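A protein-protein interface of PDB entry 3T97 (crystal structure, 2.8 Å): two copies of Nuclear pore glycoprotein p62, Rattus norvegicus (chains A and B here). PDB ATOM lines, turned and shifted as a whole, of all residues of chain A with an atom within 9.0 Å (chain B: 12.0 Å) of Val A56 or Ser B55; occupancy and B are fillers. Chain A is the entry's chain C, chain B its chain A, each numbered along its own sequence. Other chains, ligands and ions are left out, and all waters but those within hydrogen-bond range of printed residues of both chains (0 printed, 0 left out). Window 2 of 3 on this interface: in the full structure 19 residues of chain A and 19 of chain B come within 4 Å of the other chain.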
ATOM      1  N   LEU A  49      -0.397  12.878 -28.038  1.00  0.00           N
ATOM      2  CA  LEU A  49      -1.497  11.929 -28.202  1.00  0.00           C
ATOM      3  C   LEU A  49      -2.546  12.291 -29.242  1.00  0.00           C
ATOM      4  O   LEU A  49      -3.106  11.402 -29.869  1.00  0.00           O
ATOM      5  CB  LEU A  49      -2.203  11.700 -26.862  1.00  0.00           C
ATOM      6  CG  LEU A  49      -1.500  10.916 -25.760  1.00  0.00           C
ATOM      7  CD1 LEU A  49      -2.302  11.037 -24.488  1.00  0.00           C
ATOM      8  CD2 LEU A  49      -1.342   9.463 -26.180  1.00  0.00           C
ATOM      9  N   SER A  50      -2.828  13.576 -29.415  1.00  0.00           N
ATOM     10  CA  SER A  50      -3.837  14.013 -30.388  1.00  0.00           C
ATOM     11  C   SER A  50      -3.573  13.492 -31.802  1.00  0.00           C
ATOM     12  O   SER A  50      -4.499  13.093 -32.503  1.00  0.00           O
ATOM     13  CB  SER A  50      -3.939  15.545 -30.412  1.00  0.00           C
ATOM     14  OG  SER A  50      -4.518  16.047 -29.217  1.00  0.00           O
ATOM     15  N   PRO A  51      -2.305  13.507 -32.242  1.00  0.00           N
ATOM     16  CA  PRO A  51      -1.928  13.029 -33.577  1.00  0.00           C
ATOM     17  C   PRO A  51      -2.189  11.535 -33.795  1.00  0.00           C
ATOM     18  O   PRO A  51      -2.863  11.137 -34.744  1.00  0.00           O
ATOM     19  CB  PRO A  51      -0.435  13.350 -33.649  1.00  0.00           C
ATOM     20  CG  PRO A  51      -0.319  14.562 -32.796  1.00  0.00           C
ATOM     21  CD  PRO A  51      -1.175  14.204 -31.609  1.00  0.00           C
ATOM     22  N   LEU A  52      -1.650  10.713 -32.903  1.00  0.00           N
ATOM     23  CA  LEU A  52      -1.782   9.264 -33.007  1.00  0.00           C
ATOM     24  C   LEU A  52      -3.074   8.643 -32.486  1.00  0.00           C
ATOM     25  O   LEU A  52      -3.150   7.428 -32.338  1.00  0.00           O
ATOM     26  CB  LEU A  52      -0.584   8.596 -32.323  1.00  0.00           C
ATOM     27  CG  LEU A  52      -0.238   9.061 -30.908  1.00  0.00           C
ATOM     28  CD1 LEU A  52      -0.409   7.918 -29.930  1.00  0.00           C
ATOM     29  CD2 LEU A  52       1.186   9.564 -30.881  1.00  0.00           C
ATOM     30  N   GLU A  53      -4.090   9.459 -32.223  1.00  0.00           N
ATOM     31  CA  GLU A  53      -5.352   8.931 -31.712  1.00  0.00           C
ATOM     32  C   GLU A  53      -6.287   8.433 -32.822  1.00  0.00           C
ATOM     33  O   GLU A  53      -6.710   7.275 -32.818  1.00  0.00           O
ATOM     34  CB  GLU A  53      -6.082   9.994 -30.885  1.00  0.00           C
ATOM     35  CG  GLU A  53      -6.742  11.083 -31.713  1.00  0.00           C
ATOM     36  CD  GLU A  53      -7.603  12.012 -30.885  1.00  0.00           C
ATOM     37  OE1 GLU A  53      -7.036  12.853 -30.153  1.00  0.00           O
ATOM     38  OE2 GLU A  53      -8.846  11.897 -30.965  1.00  0.00           O
ATOM     39  N   GLU A  54      -6.605   9.314 -33.766  1.00  0.00           N
ATOM     40  CA  GLU A  54      -7.492   8.982 -34.874  1.00  0.00           C
ATOM     41  C   GLU A  54      -6.773   8.137 -35.936  1.00  0.00           C
ATOM     42  O   GLU A  54      -7.305   7.894 -37.023  1.00  0.00           O
ATOM     43  CB  GLU A  54      -8.041  10.284 -35.477  1.00  0.00           C
ATOM     44  CG  GLU A  54      -9.009  10.122 -36.636  1.00  0.00           C
ATOM     45  CD  GLU A  54      -9.813  11.386 -36.893  1.00  0.00           C
ATOM     46  OE1 GLU A  54      -9.277  12.489 -36.659  1.00  0.00           O
ATOM     47  OE2 GLU A  54     -10.975  11.274 -37.332  1.00  0.00           O
ATOM     48  N   SER A  55      -5.569   7.684 -35.599  1.00  0.00           N
ATOM     49  CA  SER A  55      -4.757   6.861 -36.490  1.00  0.00           C
ATOM     50  C   SER A  55      -4.750   5.407 -36.021  1.00  0.00           C
ATOM     51  O   SER A  55      -4.632   4.479 -36.825  1.00  0.00           O
ATOM     52  CB  SER A  55      -3.320   7.389 -36.533  1.00  0.00           C
ATOM     53  OG  SER A  55      -2.679   7.251 -35.273  1.00  0.00           O
ATOM     54  N   VAL A  56      -4.876   5.217 -34.710  1.00  0.00           N
ATOM     55  CA  VAL A  56      -4.889   3.886 -34.110  1.00  0.00           C
ATOM     56  C   VAL A  56      -6.309   3.352 -33.935  1.00  0.00           C
ATOM     57  O   VAL A  56      -6.532   2.176 -34.291  1.00  0.00           O
ATOM     58  CB  VAL A  56      -4.192   3.895 -32.739  1.00  0.00           C
ATOM     59  CG1 VAL A  56      -4.241   2.506 -32.112  1.00  0.00           C
ATOM     60  CG2 VAL A  56      -2.752   4.362 -32.896  1.00  0.00           C
ATOM     61  N   GLU B  46      -6.978  10.749 -20.218  1.00  0.00           N
ATOM     62  CA  GLU B  46      -7.190   9.352 -19.920  1.00  0.00           C
ATOM     63  C   GLU B  46      -8.111   8.733 -20.970  1.00  0.00           C
ATOM     64  O   GLU B  46      -7.808   7.679 -21.529  1.00  0.00           O
ATOM     65  CB  GLU B  46      -7.808   9.226 -18.538  1.00  0.00           C
ATOM     66  CG  GLU B  46      -8.248   7.824 -18.169  1.00  0.00           C
ATOM     67  CD  GLU B  46      -7.080   6.865 -17.994  1.00  0.00           C
ATOM     68  OE1 GLU B  46      -6.157   7.183 -17.209  1.00  0.00           O
ATOM     69  OE2 GLU B  46      -7.092   5.793 -18.636  1.00  0.00           O
ATOM     70  N   ASP B  47      -9.238   9.383 -21.245  1.00  0.00           N
ATOM     71  CA  ASP B  47     -10.171   8.866 -22.239  1.00  0.00           C
ATOM     72  C   ASP B  47      -9.443   8.702 -23.563  1.00  0.00           C
ATOM     73  O   ASP B  47      -9.672   7.750 -24.292  1.00  0.00           O
ATOM     74  CB  ASP B  47     -11.367   9.815 -22.444  1.00  0.00           C
ATOM     75  CG  ASP B  47     -12.203  10.015 -21.180  1.00  0.00           C
ATOM     76  OD1 ASP B  47     -12.412   9.032 -20.438  1.00  0.00           O
ATOM     77  OD2 ASP B  47     -12.669  11.154 -20.960  1.00  0.00           O
ATOM     78  N   LEU B  48      -8.552   9.641 -23.851  1.00  0.00           N
ATOM     79  CA  LEU B  48      -7.773   9.668 -25.086  1.00  0.00           C
ATOM     80  C   LEU B  48      -6.713   8.569 -25.143  1.00  0.00           C
ATOM     81  O   LEU B  48      -6.247   8.199 -26.220  1.00  0.00           O
ATOM     82  CB  LEU B  48      -7.127  11.056 -25.236  1.00  0.00           C
ATOM     83  CG  LEU B  48      -6.357  11.515 -26.483  1.00  0.00           C
ATOM     84  CD1 LEU B  48      -7.243  11.410 -27.691  1.00  0.00           C
ATOM     85  CD2 LEU B  48      -5.889  12.963 -26.307  1.00  0.00           C
ATOM     86  N   LEU B  49      -6.350   8.032 -23.986  1.00  0.00           N
ATOM     87  CA  LEU B  49      -5.325   6.993 -23.913  1.00  0.00           C
ATOM     88  C   LEU B  49      -5.839   5.570 -24.025  1.00  0.00           C
ATOM     89  O   LEU B  49      -5.249   4.756 -24.730  1.00  0.00           O
ATOM     90  CB  LEU B  49      -4.550   7.098 -22.607  1.00  0.00           C
ATOM     91  CG  LEU B  49      -3.696   8.331 -22.375  1.00  0.00           C
ATOM     92  CD1 LEU B  49      -3.141   8.285 -20.962  1.00  0.00           C
ATOM     93  CD2 LEU B  49      -2.598   8.380 -23.389  1.00  0.00           C
ATOM     94  N   SER B  50      -6.923   5.253 -23.320  1.00  0.00           N
ATOM     95  CA  SER B  50      -7.470   3.896 -23.357  1.00  0.00           C
ATOM     96  C   SER B  50      -7.525   3.326 -24.775  1.00  0.00           C
ATOM     97  O   SER B  50      -6.911   2.308 -25.054  1.00  0.00           O
ATOM     98  CB  SER B  50      -8.851   3.859 -22.701  1.00  0.00           C
ATOM     99  OG  SER B  50      -8.771   4.188 -21.319  1.00  0.00           O
ATOM    100  N   PRO B  51      -8.254   3.974 -25.688  1.00  0.00           N
ATOM    101  CA  PRO B  51      -8.332   3.471 -27.059  1.00  0.00           C
ATOM    102  C   PRO B  51      -6.989   3.124 -27.691  1.00  0.00           C
ATOM    103  O   PRO B  51      -6.868   2.115 -28.381  1.00  0.00           O
ATOM    104  CB  PRO B  51      -9.043   4.607 -27.786  1.00  0.00           C
ATOM    105  CG  PRO B  51     -10.017   5.042 -26.765  1.00  0.00           C
ATOM    106  CD  PRO B  51      -9.167   5.114 -25.512  1.00  0.00           C
ATOM    107  N   LEU B  52      -5.987   3.967 -27.452  1.00  0.00           N
ATOM    108  CA  LEU B  52      -4.644   3.757 -28.004  1.00  0.00           C
ATOM    109  C   LEU B  52      -3.893   2.590 -27.370  1.00  0.00           C
ATOM    110  O   LEU B  52      -3.216   1.840 -28.074  1.00  0.00           O
ATOM    111  CB  LEU B  52      -3.800   5.019 -27.845  1.00  0.00           C
ATOM    112  CG  LEU B  52      -4.215   6.246 -28.636  1.00  0.00           C
ATOM    113  CD1 LEU B  52      -3.373   7.419 -28.204  1.00  0.00           C
ATOM    114  CD2 LEU B  52      -4.044   5.982 -30.106  1.00  0.00           C
ATOM    115  N   GLU B  53      -3.997   2.447 -26.049  1.00  0.00           N
ATOM    116  CA  GLU B  53      -3.310   1.364 -25.358  1.00  0.00           C
ATOM    117  C   GLU B  53      -4.021   0.016 -25.479  1.00  0.00           C
ATOM    118  O   GLU B  53      -3.493  -1.020 -25.066  1.00  0.00           O
ATOM    119  CB  GLU B  53      -3.060   1.727 -23.888  1.00  0.00           C
ATOM    120  CG  GLU B  53      -4.184   2.447 -23.183  1.00  0.00           C
ATOM    121  CD  GLU B  53      -3.906   2.650 -21.695  1.00  0.00           C
ATOM    122  OE1 GLU B  53      -2.810   3.129 -21.336  1.00  0.00           O
ATOM    123  OE2 GLU B  53      -4.795   2.326 -20.881  1.00  0.00           O
ATOM    124  N   GLU B  54      -5.218   0.027 -26.056  1.00  0.00           N
ATOM    125  CA  GLU B  54      -5.980  -1.196 -26.230  1.00  0.00           C
ATOM    126  C   GLU B  54      -5.635  -1.814 -27.587  1.00  0.00           C
ATOM    127  O   GLU B  54      -5.336  -3.002 -27.672  1.00  0.00           O
ATOM    128  CB  GLU B  54      -7.488  -0.915 -26.211  1.00  0.00           C
ATOM    129  CG  GLU B  54      -8.018  -0.554 -24.830  1.00  0.00           C
ATOM    130  CD  GLU B  54      -7.700  -1.617 -23.786  1.00  0.00           C
ATOM    131  OE1 GLU B  54      -8.077  -2.791 -24.010  1.00  0.00           O
ATOM    132  OE2 GLU B  54      -7.085  -1.276 -22.745  1.00  0.00           O
ATOM    133  N   SER B  55      -5.638  -1.012 -28.643  1.00  0.00           N
ATOM    134  CA  SER B  55      -5.330  -1.523 -29.976  1.00  0.00           C
ATOM    135  C   SER B  55      -3.907  -2.051 -30.071  1.00  0.00           C
ATOM    136  O   SER B  55      -3.519  -2.623 -31.095  1.00  0.00           O
ATOM    137  CB  SER B  55      -5.438  -0.351 -30.991  1.00  0.00           C
ATOM    138  OG  SER B  55      -6.669   0.352 -30.846  1.00  0.00           O
ATOM    139  N   VAL B  56      -3.177  -1.950 -28.972  1.00  0.00           N
ATOM    140  CA  VAL B  56      -1.811  -2.443 -28.915  1.00  0.00           C
ATOM    141  C   VAL B  56      -1.512  -3.483 -27.873  1.00  0.00           C
ATOM    142  O   VAL B  56      -0.377  -3.928 -27.739  1.00  0.00           O
ATOM    143  CB  VAL B  56      -0.905  -1.193 -28.665  1.00  0.00           C
ATOM    144  CG1 VAL B  56      -1.037  -0.744 -27.204  1.00  0.00           C
ATOM    145  CG2 VAL B  56       0.536  -1.493 -29.011  1.00  0.00           C
ATOM    146  N   LYS B  57      -2.536  -3.864 -27.128  1.00  0.00           N
ATOM    147  CA  LYS B  57      -2.395  -4.868 -26.075  1.00  0.00           C
ATOM    148  C   LYS B  57      -2.236  -6.258 -26.676  1.00  0.00           C
ATOM    149  O   LYS B  57      -2.833  -7.222 -26.203  1.00  0.00           O
ATOM    150  CB  LYS B  57      -3.622  -4.860 -25.154  1.00  0.00           C
ATOM    151  CG  LYS B  57      -4.894  -5.377 -25.819  1.00  0.00           C
ATOM    152  CD  LYS B  57      -6.099  -5.266 -24.897  1.00  0.00           C
ATOM    153  CE  LYS B  57      -7.360  -5.737 -25.607  1.00  0.00           C
ATOM    154  NZ  LYS B  57      -8.586  -5.460 -24.808  1.00  0.00           N
ATOM    155  N   GLU B  58      -1.420  -6.350 -27.720  1.00  0.00           N
ATOM    156  CA  GLU B  58      -1.172  -7.616 -28.401  1.00  0.00           C
ATOM    157  C   GLU B  58       0.019  -8.373 -27.817  1.00  0.00           C
ATOM    158  O   GLU B  58      -0.158  -9.560 -27.471  1.00  0.00           O
ATOM    159  CB  GLU B  58      -0.957  -7.366 -29.895  1.00  0.00           C
ATOM    160  CG  GLU B  58      -2.123  -6.648 -30.547  1.00  0.00           C
ATOM    161  CD  GLU B  58      -1.974  -6.525 -32.045  1.00  0.00           C
ATOM    162  OE1 GLU B  58      -0.951  -5.968 -32.495  1.00  0.00           O
ATOM    163  OE2 GLU B  58      -2.879  -6.980 -32.774  1.00  0.00           O
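Of the 13 printed residues of chain B, 4 touch a printed residue of chain A. Of the 8 printed residues of chain A, 4 touch a printed residue of chain B. Among the printed residues, 8 pairs touch across the chains.
Among the printed residues, merely in contact across the chains: Leu A49 with Leu B48, Leu A49 with Leu B49, Leu A49 with Leu B52, Leu A52 with Leu B52, Glu A53 with Leu B48, Glu A53 with Leu B52, Val A56 with Leu B52 and Val A56 with Ser B55.
Leu A49 touches its own counterpart, Leu B49. Leu A49 touches Leu B52, but with the chains exchanged Leu A52 does not touch Leu B49 (6.9 Å). Leu B52 touches its own counterpart, Leu A52. Val A56 touches Leu B52, but with the chains exchanged Leu A52 does not touch Val B56 (9.1 Å).
Of chain B, only Leu B52 (3.4 Å) and Ser B55 (3.3 Å) come within 4 Å of Val A56. Ser B55 touches just one residue of chain A: Val A56 (3.3 Å). Leu A52 touches one residue of chain B. No residue of chain B comes within 4 Å of Ser A55. Of the printed residues of chain B, Leu A49 touches Leu B48 (3.9 Å), Leu B49 (2.9 Å) and Leu B52 (3.5 Å). Printed residues of chain A within 4 Å of Leu B48: Leu A49 and Glu A53. The nearest residue of chain A that does not touch Ser B55 is Glu A53 (7.2 Å). The nearest printed residue of chain A that does not touch Leu B49 is Leu A52 (6.9 Å).
OG of Ser A55 is in hydrogen-bond range of O of Leu A52, at 3.0 Å. O of Pro B51 is in hydrogen-bond range of OG of Ser B55, 3.0 Å away.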
